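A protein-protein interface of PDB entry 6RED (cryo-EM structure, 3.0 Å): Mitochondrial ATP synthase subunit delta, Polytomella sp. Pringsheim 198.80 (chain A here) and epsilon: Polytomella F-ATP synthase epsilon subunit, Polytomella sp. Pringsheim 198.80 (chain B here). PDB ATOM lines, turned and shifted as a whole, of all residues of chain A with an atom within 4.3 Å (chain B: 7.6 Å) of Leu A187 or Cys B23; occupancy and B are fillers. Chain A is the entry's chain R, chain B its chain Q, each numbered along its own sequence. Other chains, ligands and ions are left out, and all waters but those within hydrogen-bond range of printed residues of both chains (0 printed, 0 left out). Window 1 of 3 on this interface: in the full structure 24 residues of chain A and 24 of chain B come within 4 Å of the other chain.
Hydrophobic or aromatic side chains of chain A that line the printed part of chain B: Phe A128, Ala A183, Ala A184, Leu A187, Tyr A188 and Leu A191.
Printed residues of chain B that touch a printed residue of chain A: Tyr B19, Cys B23, Ala B24, Leu B26, Leu B27 and Val B30.
Hydrophobic or aromatic side chains of chain B within 4 Å of the printed part of chain A: Tyr B19, Ala B24, Leu B26, Leu B27 and Val B30.
Along chain B the printed residues that touch a printed residue of chain A span positions 19 to 30.
Among the printed residues, 13 pairs touch across the chains.
Among the printed residues, no Asp or Glu carboxylate lies within 4 Å of a Lys or Arg side-chain nitrogen of the other chain.
Cys B23 touches three residues of chain A.
Printed residues of chain B within 4 Å of Leu A191: Val B30 (3.7 Å).
Printed residues of chain A within 4 Å of Tyr B19: Ala A183 (3.7 Å).
Printed residues of chain B within 4 Å of Tyr A188: Leu B26 (2.9 Å) and Val B30 (3.6 Å).
Of the printed residues of chain A, Leu B27 touches Phe A128 (3.6 Å), Ser A130 (3.7 Å) and Leu A187 (3.5 Å).
Of the printed residues of chain A, Ala B24 touches Ser A130.
The nearest printed residue of chain A that does not touch Cys B23 is Pro A113 (5.0 Å).
The backbone carbonyl oxygen of Leu B26 sits at hydrogen-bond distance from the side-chain hydroxyl of Tyr A188, 2.9 Å away.
The backbone carbonyl oxygen (O) of Tyr B19 is in hydrogen-bond range of the side-chain sulfur (SG) of Cys B23 (3.5 Å).
Among the printed residues, pairs that only touch across the chains: Phe A128 with Leu B27, Ser A130 with Cys B23, Ser A130 with Ala B24, Ser A130 with Leu B27, Ala A183 with Tyr B19, Ala A183 with Cys B23, Ala A184 with Leu B26, Leu A187 with Cys B23, Leu A187 with Leu B26, Leu A187 with Leu B27, Tyr A188 with Val B30 and Leu A191 with Val B30.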
ATOM      1  N   PRO A 113      23.681 -36.788 -25.983  1.00  0.00           N
ATOM      2  CA  PRO A 113      24.323 -37.227 -27.228  1.00  0.00           C
ATOM      3  C   PRO A 113      24.737 -38.688 -27.204  1.00  0.00           C
ATOM      4  O   PRO A 113      25.465 -39.130 -26.320  1.00  0.00           O
ATOM      5  CB  PRO A 113      25.538 -36.315 -27.320  1.00  0.00           C
ATOM      6  CG  PRO A 113      25.107 -35.092 -26.699  1.00  0.00           C
ATOM      7  CD  PRO A 113      24.170 -35.447 -25.602  1.00  0.00           C
ATOM      8  N   PHE A 128      23.360 -41.522 -34.922  1.00  0.00           N
ATOM      9  CA  PHE A 128      23.909 -40.764 -33.813  1.00  0.00           C
ATOM     10  C   PHE A 128      23.186 -39.434 -33.720  1.00  0.00           C
ATOM     11  O   PHE A 128      23.141 -38.683 -34.693  1.00  0.00           O
ATOM     12  CB  PHE A 128      25.404 -40.531 -33.987  1.00  0.00           C
ATOM     13  CG  PHE A 128      26.022 -39.783 -32.856  1.00  0.00           C
ATOM     14  CD1 PHE A 128      26.368 -40.433 -31.695  1.00  0.00           C
ATOM     15  CD2 PHE A 128      26.253 -38.435 -32.946  1.00  0.00           C
ATOM     16  CE1 PHE A 128      26.928 -39.745 -30.652  1.00  0.00           C
ATOM     17  CE2 PHE A 128      26.808 -37.753 -31.912  1.00  0.00           C
ATOM     18  CZ  PHE A 128      27.144 -38.404 -30.764  1.00  0.00           C
ATOM     19  N   SER A 130      22.097 -35.731 -31.410  1.00  0.00           N
ATOM     20  CA  SER A 130      22.788 -34.647 -30.734  1.00  0.00           C
ATOM     21  C   SER A 130      22.148 -34.247 -29.418  1.00  0.00           C
ATOM     22  O   SER A 130      22.693 -33.392 -28.719  1.00  0.00           O
ATOM     23  CB  SER A 130      22.853 -33.423 -31.642  1.00  0.00           C
ATOM     24  OG  SER A 130      21.554 -32.934 -31.899  1.00  0.00           O
ATOM     25  N   ALA A 183      28.871 -29.004 -23.206  1.00  0.00           N
ATOM     26  CA  ALA A 183      28.083 -29.635 -24.261  1.00  0.00           C
ATOM     27  C   ALA A 183      28.972 -30.178 -25.374  1.00  0.00           C
ATOM     28  O   ALA A 183      28.729 -31.273 -25.896  1.00  0.00           O
ATOM     29  CB  ALA A 183      27.083 -28.636 -24.827  1.00  0.00           C
ATOM     30  N   ALA A 184      30.033 -29.436 -25.706  1.00  0.00           N
ATOM     31  CA  ALA A 184      30.975 -29.856 -26.737  1.00  0.00           C
ATOM     32  C   ALA A 184      31.698 -31.130 -26.342  1.00  0.00           C
ATOM     33  O   ALA A 184      31.776 -32.082 -27.127  1.00  0.00           O
ATOM     34  CB  ALA A 184      31.987 -28.746 -26.995  1.00  0.00           C
ATOM     35  N   ILE A 185      32.234 -31.170 -25.123  1.00  0.00           N
ATOM     36  CA  ILE A 185      33.035 -32.323 -24.736  1.00  0.00           C
ATOM     37  C   ILE A 185      32.156 -33.538 -24.487  1.00  0.00           C
ATOM     38  O   ILE A 185      32.559 -34.660 -24.808  1.00  0.00           O
ATOM     39  CB  ILE A 185      33.941 -31.982 -23.540  1.00  0.00           C
ATOM     40  CG1 ILE A 185      33.142 -31.580 -22.308  1.00  0.00           C
ATOM     41  CG2 ILE A 185      34.880 -30.862 -23.913  1.00  0.00           C
ATOM     42  CD1 ILE A 185      34.000 -31.418 -21.070  1.00  0.00           C
ATOM     43  N   GLU A 186      30.916 -33.333 -24.016  1.00  0.00           N
ATOM     44  CA  GLU A 186      29.954 -34.427 -23.899  1.00  0.00           C
ATOM     45  C   GLU A 186      29.621 -35.029 -25.256  1.00  0.00           C
ATOM     46  O   GLU A 186      29.721 -36.252 -25.437  1.00  0.00           O
ATOM     47  CB  GLU A 186      28.678 -33.918 -23.233  1.00  0.00           C
ATOM     48  CG  GLU A 186      28.747 -33.808 -21.731  1.00  0.00           C
ATOM     49  CD  GLU A 186      27.392 -33.951 -21.085  1.00  0.00           C
ATOM     50  OE1 GLU A 186      26.537 -34.658 -21.657  1.00  0.00           O
ATOM     51  OE2 GLU A 186      27.178 -33.347 -20.011  1.00  0.00           O
ATOM     52  N   LEU A 187      29.267 -34.180 -26.229  1.00  0.00           N
ATOM     53  CA  LEU A 187      28.854 -34.671 -27.537  1.00  0.00           C
ATOM     54  C   LEU A 187      30.011 -35.321 -28.273  1.00  0.00           C
ATOM     55  O   LEU A 187      29.864 -36.408 -28.841  1.00  0.00           O
ATOM     56  CB  LEU A 187      28.271 -33.530 -28.364  1.00  0.00           C
ATOM     57  CG  LEU A 187      28.200 -33.729 -29.872  1.00  0.00           C
ATOM     58  CD1 LEU A 187      27.088 -34.645 -30.219  1.00  0.00           C
ATOM     59  CD2 LEU A 187      27.970 -32.417 -30.525  1.00  0.00           C
ATOM     60  N   TYR A 188      31.185 -34.688 -28.237  1.00  0.00           N
ATOM     61  CA  TYR A 188      32.322 -35.216 -28.972  1.00  0.00           C
ATOM     62  C   TYR A 188      32.857 -36.481 -28.330  1.00  0.00           C
ATOM     63  O   TYR A 188      33.243 -37.407 -29.038  1.00  0.00           O
ATOM     64  CB  TYR A 188      33.411 -34.159 -29.075  1.00  0.00           C
ATOM     65  CG  TYR A 188      33.090 -33.077 -30.064  1.00  0.00           C
ATOM     66  CD1 TYR A 188      32.404 -33.363 -31.230  1.00  0.00           C
ATOM     67  CD2 TYR A 188      33.468 -31.767 -29.830  1.00  0.00           C
ATOM     68  CE1 TYR A 188      32.107 -32.382 -32.133  1.00  0.00           C
ATOM     69  CE2 TYR A 188      33.173 -30.776 -30.732  1.00  0.00           C
ATOM     70  CZ  TYR A 188      32.493 -31.089 -31.883  1.00  0.00           C
ATOM     71  OH  TYR A 188      32.200 -30.095 -32.784  1.00  0.00           O
ATOM     72  N   SER A 189      32.843 -36.564 -26.998  1.00  0.00           N
ATOM     73  CA  SER A 189      33.309 -37.772 -26.336  1.00  0.00           C
ATOM     74  C   SER A 189      32.379 -38.942 -26.582  1.00  0.00           C
ATOM     75  O   SER A 189      32.848 -40.060 -26.835  1.00  0.00           O
ATOM     76  CB  SER A 189      33.426 -37.522 -24.847  1.00  0.00           C
ATOM     77  OG  SER A 189      32.251 -36.903 -24.367  1.00  0.00           O
ATOM     78  N   ALA A 190      31.067 -38.708 -26.526  1.00  0.00           N
ATOM     79  CA  ALA A 190      30.134 -39.780 -26.828  1.00  0.00           C
ATOM     80  C   ALA A 190      30.185 -40.165 -28.293  1.00  0.00           C
ATOM     81  O   ALA A 190      29.921 -41.320 -28.636  1.00  0.00           O
ATOM     82  CB  ALA A 190      28.727 -39.361 -26.438  1.00  0.00           C
ATOM     83  N   LEU A 191      30.548 -39.232 -29.164  1.00  0.00           N
ATOM     84  CA  LEU A 191      30.706 -39.575 -30.566  1.00  0.00           C
ATOM     85  C   LEU A 191      31.963 -40.389 -30.802  1.00  0.00           C
ATOM     86  O   LEU A 191      31.949 -41.314 -31.617  1.00  0.00           O
ATOM     87  CB  LEU A 191      30.718 -38.300 -31.407  1.00  0.00           C
ATOM     88  CG  LEU A 191      30.793 -38.458 -32.916  1.00  0.00           C
ATOM     89  CD1 LEU A 191      29.754 -39.440 -33.410  1.00  0.00           C
ATOM     90  CD2 LEU A 191      30.574 -37.113 -33.532  1.00  0.00           C
ATOM     91  N   PHE B   8      22.471 -27.683 -16.495  1.00  0.00           N
ATOM     92  CA  PHE B   8      23.707 -26.906 -16.495  1.00  0.00           C
ATOM     93  C   PHE B   8      23.663 -25.750 -17.479  1.00  0.00           C
ATOM     94  O   PHE B   8      24.277 -24.707 -17.230  1.00  0.00           O
ATOM     95  CB  PHE B   8      24.902 -27.806 -16.791  1.00  0.00           C
ATOM     96  CG  PHE B   8      24.928 -28.383 -18.181  1.00  0.00           C
ATOM     97  CD1 PHE B   8      25.678 -27.790 -19.181  1.00  0.00           C
ATOM     98  CD2 PHE B   8      24.243 -29.546 -18.473  1.00  0.00           C
ATOM     99  CE1 PHE B   8      25.718 -28.322 -20.439  1.00  0.00           C
ATOM    100  CE2 PHE B   8      24.284 -30.082 -19.736  1.00  0.00           C
ATOM    101  CZ  PHE B   8      25.024 -29.469 -20.718  1.00  0.00           C
ATOM    102  N   TYR B   9      22.968 -25.915 -18.598  1.00  0.00           N
ATOM    103  CA  TYR B   9      22.730 -24.783 -19.478  1.00  0.00           C
ATOM    104  C   TYR B   9      21.788 -23.785 -18.829  1.00  0.00           C
ATOM    105  O   TYR B   9      21.952 -22.575 -19.007  1.00  0.00           O
ATOM    106  CB  TYR B   9      22.171 -25.261 -20.819  1.00  0.00           C
ATOM    107  CG  TYR B   9      21.026 -26.244 -20.729  1.00  0.00           C
ATOM    108  CD1 TYR B   9      21.256 -27.607 -20.760  1.00  0.00           C
ATOM    109  CD2 TYR B   9      19.716 -25.811 -20.645  1.00  0.00           C
ATOM    110  CE1 TYR B   9      20.222 -28.499 -20.684  1.00  0.00           C
ATOM    111  CE2 TYR B   9      18.678 -26.697 -20.568  1.00  0.00           C
ATOM    112  CZ  TYR B   9      18.937 -28.036 -20.590  1.00  0.00           C
ATOM    113  OH  TYR B   9      17.898 -28.924 -20.518  1.00  0.00           O
ATOM    114  N   MET B  14      21.613 -20.020 -20.508  1.00  0.00           N
ATOM    115  CA  MET B  14      21.435 -20.607 -21.824  1.00  0.00           C
ATOM    116  C   MET B  14      20.127 -21.384 -21.861  1.00  0.00           C
ATOM    117  O   MET B  14      19.876 -22.229 -21.002  1.00  0.00           O
ATOM    118  CB  MET B  14      22.621 -21.514 -22.144  1.00  0.00           C
ATOM    119  CG  MET B  14      22.540 -22.232 -23.456  1.00  0.00           C
ATOM    120  SD  MET B  14      23.840 -23.460 -23.642  1.00  0.00           S
ATOM    121  CE  MET B  14      25.254 -22.428 -23.949  1.00  0.00           C
ATOM    122  N   LEU B  17      16.706 -24.172 -26.191  1.00  0.00           N
ATOM    123  CA  LEU B  17      16.806 -24.081 -27.637  1.00  0.00           C
ATOM    124  C   LEU B  17      18.216 -23.728 -28.062  1.00  0.00           C
ATOM    125  O   LEU B  17      18.744 -24.311 -29.015  1.00  0.00           O
ATOM    126  CB  LEU B  17      15.815 -23.054 -28.160  1.00  0.00           C
ATOM    127  CG  LEU B  17      14.414 -23.610 -28.313  1.00  0.00           C
ATOM    128  CD1 LEU B  17      13.509 -22.532 -28.826  1.00  0.00           C
ATOM    129  CD2 LEU B  17      14.445 -24.779 -29.263  1.00  0.00           C
ATOM    130  N   ARG B  18      18.850 -22.807 -27.338  1.00  0.00           N
ATOM    131  CA  ARG B  18      20.229 -22.450 -27.637  1.00  0.00           C
ATOM    132  C   ARG B  18      21.165 -23.616 -27.380  1.00  0.00           C
ATOM    133  O   ARG B  18      22.049 -23.888 -28.195  1.00  0.00           O
ATOM    134  CB  ARG B  18      20.654 -21.246 -26.812  1.00  0.00           C
ATOM    135  CG  ARG B  18      22.013 -20.733 -27.196  1.00  0.00           C
ATOM    136  CD  ARG B  18      22.290 -19.407 -26.553  1.00  0.00           C
ATOM    137  NE  ARG B  18      21.286 -18.421 -26.915  1.00  0.00           N
ATOM    138  CZ  ARG B  18      21.362 -17.650 -27.988  1.00  0.00           C
ATOM    139  NH1 ARG B  18      22.397 -17.752 -28.807  1.00  0.00           N
ATOM    140  NH2 ARG B  18      20.403 -16.779 -28.245  1.00  0.00           N
ATOM    141  N   TYR B  19      20.949 -24.341 -26.281  1.00  0.00           N
ATOM    142  CA  TYR B  19      21.782 -25.492 -25.949  1.00  0.00           C
ATOM    143  C   TYR B  19      21.646 -26.600 -26.985  1.00  0.00           C
ATOM    144  O   TYR B  19      22.647 -27.149 -27.464  1.00  0.00           O
ATOM    145  CB  TYR B  19      21.404 -26.011 -24.564  1.00  0.00           C
ATOM    146  CG  TYR B  19      21.827 -27.431 -24.320  1.00  0.00           C
ATOM    147  CD1 TYR B  19      20.896 -28.454 -24.278  1.00  0.00           C
ATOM    148  CD2 TYR B  19      23.163 -27.749 -24.129  1.00  0.00           C
ATOM    149  CE1 TYR B  19      21.282 -29.747 -24.066  1.00  0.00           C
ATOM    150  CE2 TYR B  19      23.553 -29.037 -23.907  1.00  0.00           C
ATOM    151  CZ  TYR B  19      22.611 -30.033 -23.882  1.00  0.00           C
ATOM    152  OH  TYR B  19      22.999 -31.329 -23.662  1.00  0.00           O
ATOM    153  N   SER B  20      20.410 -26.944 -27.337  1.00  0.00           N
ATOM    154  CA  SER B  20      20.181 -28.032 -28.270  1.00  0.00           C
ATOM    155  C   SER B  20      20.626 -27.671 -29.675  1.00  0.00           C
ATOM    156  O   SER B  20      21.141 -28.531 -30.398  1.00  0.00           O
ATOM    157  CB  SER B  20      18.711 -28.424 -28.250  1.00  0.00           C
ATOM    158  OG  SER B  20      17.905 -27.345 -28.670  1.00  0.00           O
ATOM    159  N   ASN B  21      20.504 -26.400 -30.065  1.00  0.00           N
ATOM    160  CA  ASN B  21      21.011 -26.014 -31.373  1.00  0.00           C
ATOM    161  C   ASN B  21      22.526 -25.949 -31.385  1.00  0.00           C
ATOM    162  O   ASN B  21      23.136 -26.227 -32.416  1.00  0.00           O
ATOM    163  CB  ASN B  21      20.414 -24.683 -31.804  1.00  0.00           C
ATOM    164  CG  ASN B  21      19.036 -24.834 -32.376  1.00  0.00           C
ATOM    165  OD1 ASN B  21      18.869 -25.248 -33.515  1.00  0.00           O
ATOM    166  ND2 ASN B  21      18.035 -24.511 -31.584  1.00  0.00           N
ATOM    167  N   ILE B  22      23.146 -25.607 -30.254  1.00  0.00           N
ATOM    168  CA  ILE B  22      24.602 -25.653 -30.149  1.00  0.00           C
ATOM    169  C   ILE B  22      25.096 -27.086 -30.309  1.00  0.00           C
ATOM    170  O   ILE B  22      26.038 -27.345 -31.064  1.00  0.00           O
ATOM    171  CB  ILE B  22      25.051 -25.023 -28.818  1.00  0.00           C
ATOM    172  CG1 ILE B  22      25.192 -23.518 -28.987  1.00  0.00           C
ATOM    173  CG2 ILE B  22      26.364 -25.585 -28.336  1.00  0.00           C
ATOM    174  CD1 ILE B  22      25.256 -22.779 -27.699  1.00  0.00           C
ATOM    175  N   CYS B  23      24.423 -28.037 -29.650  1.00  0.00           N
ATOM    176  CA  CYS B  23      24.764 -29.452 -29.804  1.00  0.00           C
ATOM    177  C   CYS B  23      24.562 -29.931 -31.231  1.00  0.00           C
ATOM    178  O   CYS B  23      25.379 -30.695 -31.756  1.00  0.00           O
ATOM    179  CB  CYS B  23      23.928 -30.307 -28.860  1.00  0.00           C
ATOM    180  SG  CYS B  23      24.335 -30.150 -27.137  1.00  0.00           S
ATOM    181  N   ALA B  24      23.492 -29.473 -31.883  1.00  0.00           N
ATOM    182  CA  ALA B  24      23.230 -29.881 -33.259  1.00  0.00           C
ATOM    183  C   ALA B  24      24.266 -29.308 -34.209  1.00  0.00           C
ATOM    184  O   ALA B  24      24.706 -29.992 -35.140  1.00  0.00           O
ATOM    185  CB  ALA B  24      21.829 -29.451 -33.667  1.00  0.00           C
ATOM    186  N   ASP B  25      24.693 -28.068 -33.963  1.00  0.00           N
ATOM    187  CA  ASP B  25      25.717 -27.438 -34.787  1.00  0.00           C
ATOM    188  C   ASP B  25      27.052 -28.140 -34.638  1.00  0.00           C
ATOM    189  O   ASP B  25      27.730 -28.407 -35.632  1.00  0.00           O
ATOM    190  CB  ASP B  25      25.864 -25.970 -34.407  1.00  0.00           C
ATOM    191  CG  ASP B  25      24.708 -25.132 -34.880  1.00  0.00           C
ATOM    192  OD1 ASP B  25      24.518 -24.029 -34.328  1.00  0.00           O
ATOM    193  OD2 ASP B  25      23.972 -25.585 -35.778  1.00  0.00           O
ATOM    194  N   LEU B  26      27.436 -28.462 -33.403  1.00  0.00           N
ATOM    195  CA  LEU B  26      28.696 -29.152 -33.173  1.00  0.00           C
ATOM    196  C   LEU B  26      28.665 -30.593 -33.642  1.00  0.00           C
ATOM    197  O   LEU B  26      29.726 -31.164 -33.893  1.00  0.00           O
ATOM    198  CB  LEU B  26      29.068 -29.100 -31.697  1.00  0.00           C
ATOM    199  CG  LEU B  26      29.226 -27.691 -31.140  1.00  0.00           C
ATOM    200  CD1 LEU B  26      29.637 -27.744 -29.693  1.00  0.00           C
ATOM    201  CD2 LEU B  26      30.204 -26.872 -31.963  1.00  0.00           C
ATOM    202  N   LEU B  27      27.493 -31.200 -33.761  1.00  0.00           N
ATOM    203  CA  LEU B  27      27.440 -32.468 -34.469  1.00  0.00           C
ATOM    204  C   LEU B  27      27.617 -32.260 -35.964  1.00  0.00           C
ATOM    205  O   LEU B  27      28.274 -33.065 -36.626  1.00  0.00           O
ATOM    206  CB  LEU B  27      26.124 -33.191 -34.188  1.00  0.00           C
ATOM    207  CG  LEU B  27      25.833 -34.463 -34.982  1.00  0.00           C
ATOM    208  CD1 LEU B  27      26.939 -35.473 -34.811  1.00  0.00           C
ATOM    209  CD2 LEU B  27      24.535 -35.058 -34.555  1.00  0.00           C
ATOM    210  N   ARG B  28      27.050 -31.182 -36.509  1.00  0.00           N
ATOM    211  CA  ARG B  28      27.107 -30.977 -37.953  1.00  0.00           C
ATOM    212  C   ARG B  28      28.511 -30.666 -38.457  1.00  0.00           C
ATOM    213  O   ARG B  28      28.798 -30.923 -39.626  1.00  0.00           O
ATOM    214  CB  ARG B  28      26.164 -29.852 -38.367  1.00  0.00           C
ATOM    215  CG  ARG B  28      24.694 -30.224 -38.401  1.00  0.00           C
ATOM    216  CD  ARG B  28      23.881 -29.089 -38.976  1.00  0.00           C
ATOM    217  NE  ARG B  28      22.527 -29.046 -38.444  1.00  0.00           N
ATOM    218  CZ  ARG B  28      22.089 -28.106 -37.621  1.00  0.00           C
ATOM    219  NH1 ARG B  28      22.900 -27.136 -37.239  1.00  0.00           N
ATOM    220  NH2 ARG B  28      20.842 -28.132 -37.180  1.00  0.00           N
ATOM    221  N   ASN B  29      29.391 -30.143 -37.604  1.00  0.00           N
ATOM    222  CA  ASN B  29      30.718 -29.735 -38.044  1.00  0.00           C
ATOM    223  C   ASN B  29      31.637 -30.911 -38.328  1.00  0.00           C
ATOM    224  O   ASN B  29      32.580 -30.767 -39.109  1.00  0.00           O
ATOM    225  CB  ASN B  29      31.359 -28.837 -36.997  1.00  0.00           C
ATOM    226  CG  ASN B  29      30.659 -27.518 -36.877  1.00  0.00           C
ATOM    227  OD1 ASN B  29      29.657 -27.285 -37.541  1.00  0.00           O
ATOM    228  ND2 ASN B  29      31.183 -26.639 -36.038  1.00  0.00           N
ATOM    229  N   VAL B  30      31.392 -32.061 -37.722  1.00  0.00           N
ATOM    230  CA  VAL B  30      32.305 -33.183 -37.820  1.00  0.00           C
ATOM    231  C   VAL B  30      31.819 -34.221 -38.829  1.00  0.00           C
ATOM    232  O   VAL B  30      32.262 -35.367 -38.800  1.00  0.00           O
ATOM    233  CB  VAL B  30      32.558 -33.815 -36.447  1.00  0.00           C
ATOM    234  CG1 VAL B  30      33.176 -32.799 -35.535  1.00  0.00           C
ATOM    235  CG2 VAL B  30      31.272 -34.307 -35.859  1.00  0.00           C
ATOM    236  N   ILE B  69      23.964 -21.089 -34.513  1.00  0.00           N
ATOM    237  CA  ILE B  69      23.374 -20.278 -33.450  1.00  0.00           C
ATOM    238  C   ILE B  69      24.552 -19.735 -32.643  1.00  0.00           C
ATOM    239  O   ILE B  69      25.601 -20.393 -32.583  1.00  0.00           O
ATOM    240  CB  ILE B  69      22.355 -21.111 -32.639  1.00  0.00           C
ATOM    241  CG1 ILE B  69      21.329 -20.237 -31.914  1.00  0.00           C
ATOM    242  CG2 ILE B  69      23.025 -22.049 -31.658  1.00  0.00           C
ATOM    243  CD1 ILE B  69      20.147 -20.980 -31.379  1.00  0.00           C
ATOM    244  N   LYS B  71      27.121 -19.305 -30.055  1.00  0.00           N
ATOM    245  CA  LYS B  71      27.579 -19.980 -28.849  1.00  0.00           C
ATOM    246  C   LYS B  71      28.078 -19.019 -27.787  1.00  0.00           C
ATOM    247  O   LYS B  71      28.167 -19.405 -26.618  1.00  0.00           O
ATOM    248  CB  LYS B  71      28.685 -20.974 -29.189  1.00  0.00           C
ATOM    249  CG  LYS B  71      28.329 -21.887 -30.321  1.00  0.00           C
ATOM    250  CD  LYS B  71      29.512 -22.706 -30.760  1.00  0.00           C
ATOM    251  CE  LYS B  71      29.258 -23.266 -32.143  1.00  0.00           C
ATOM    252  NZ  LYS B  71      28.858 -22.183 -33.091  1.00  0.00           N
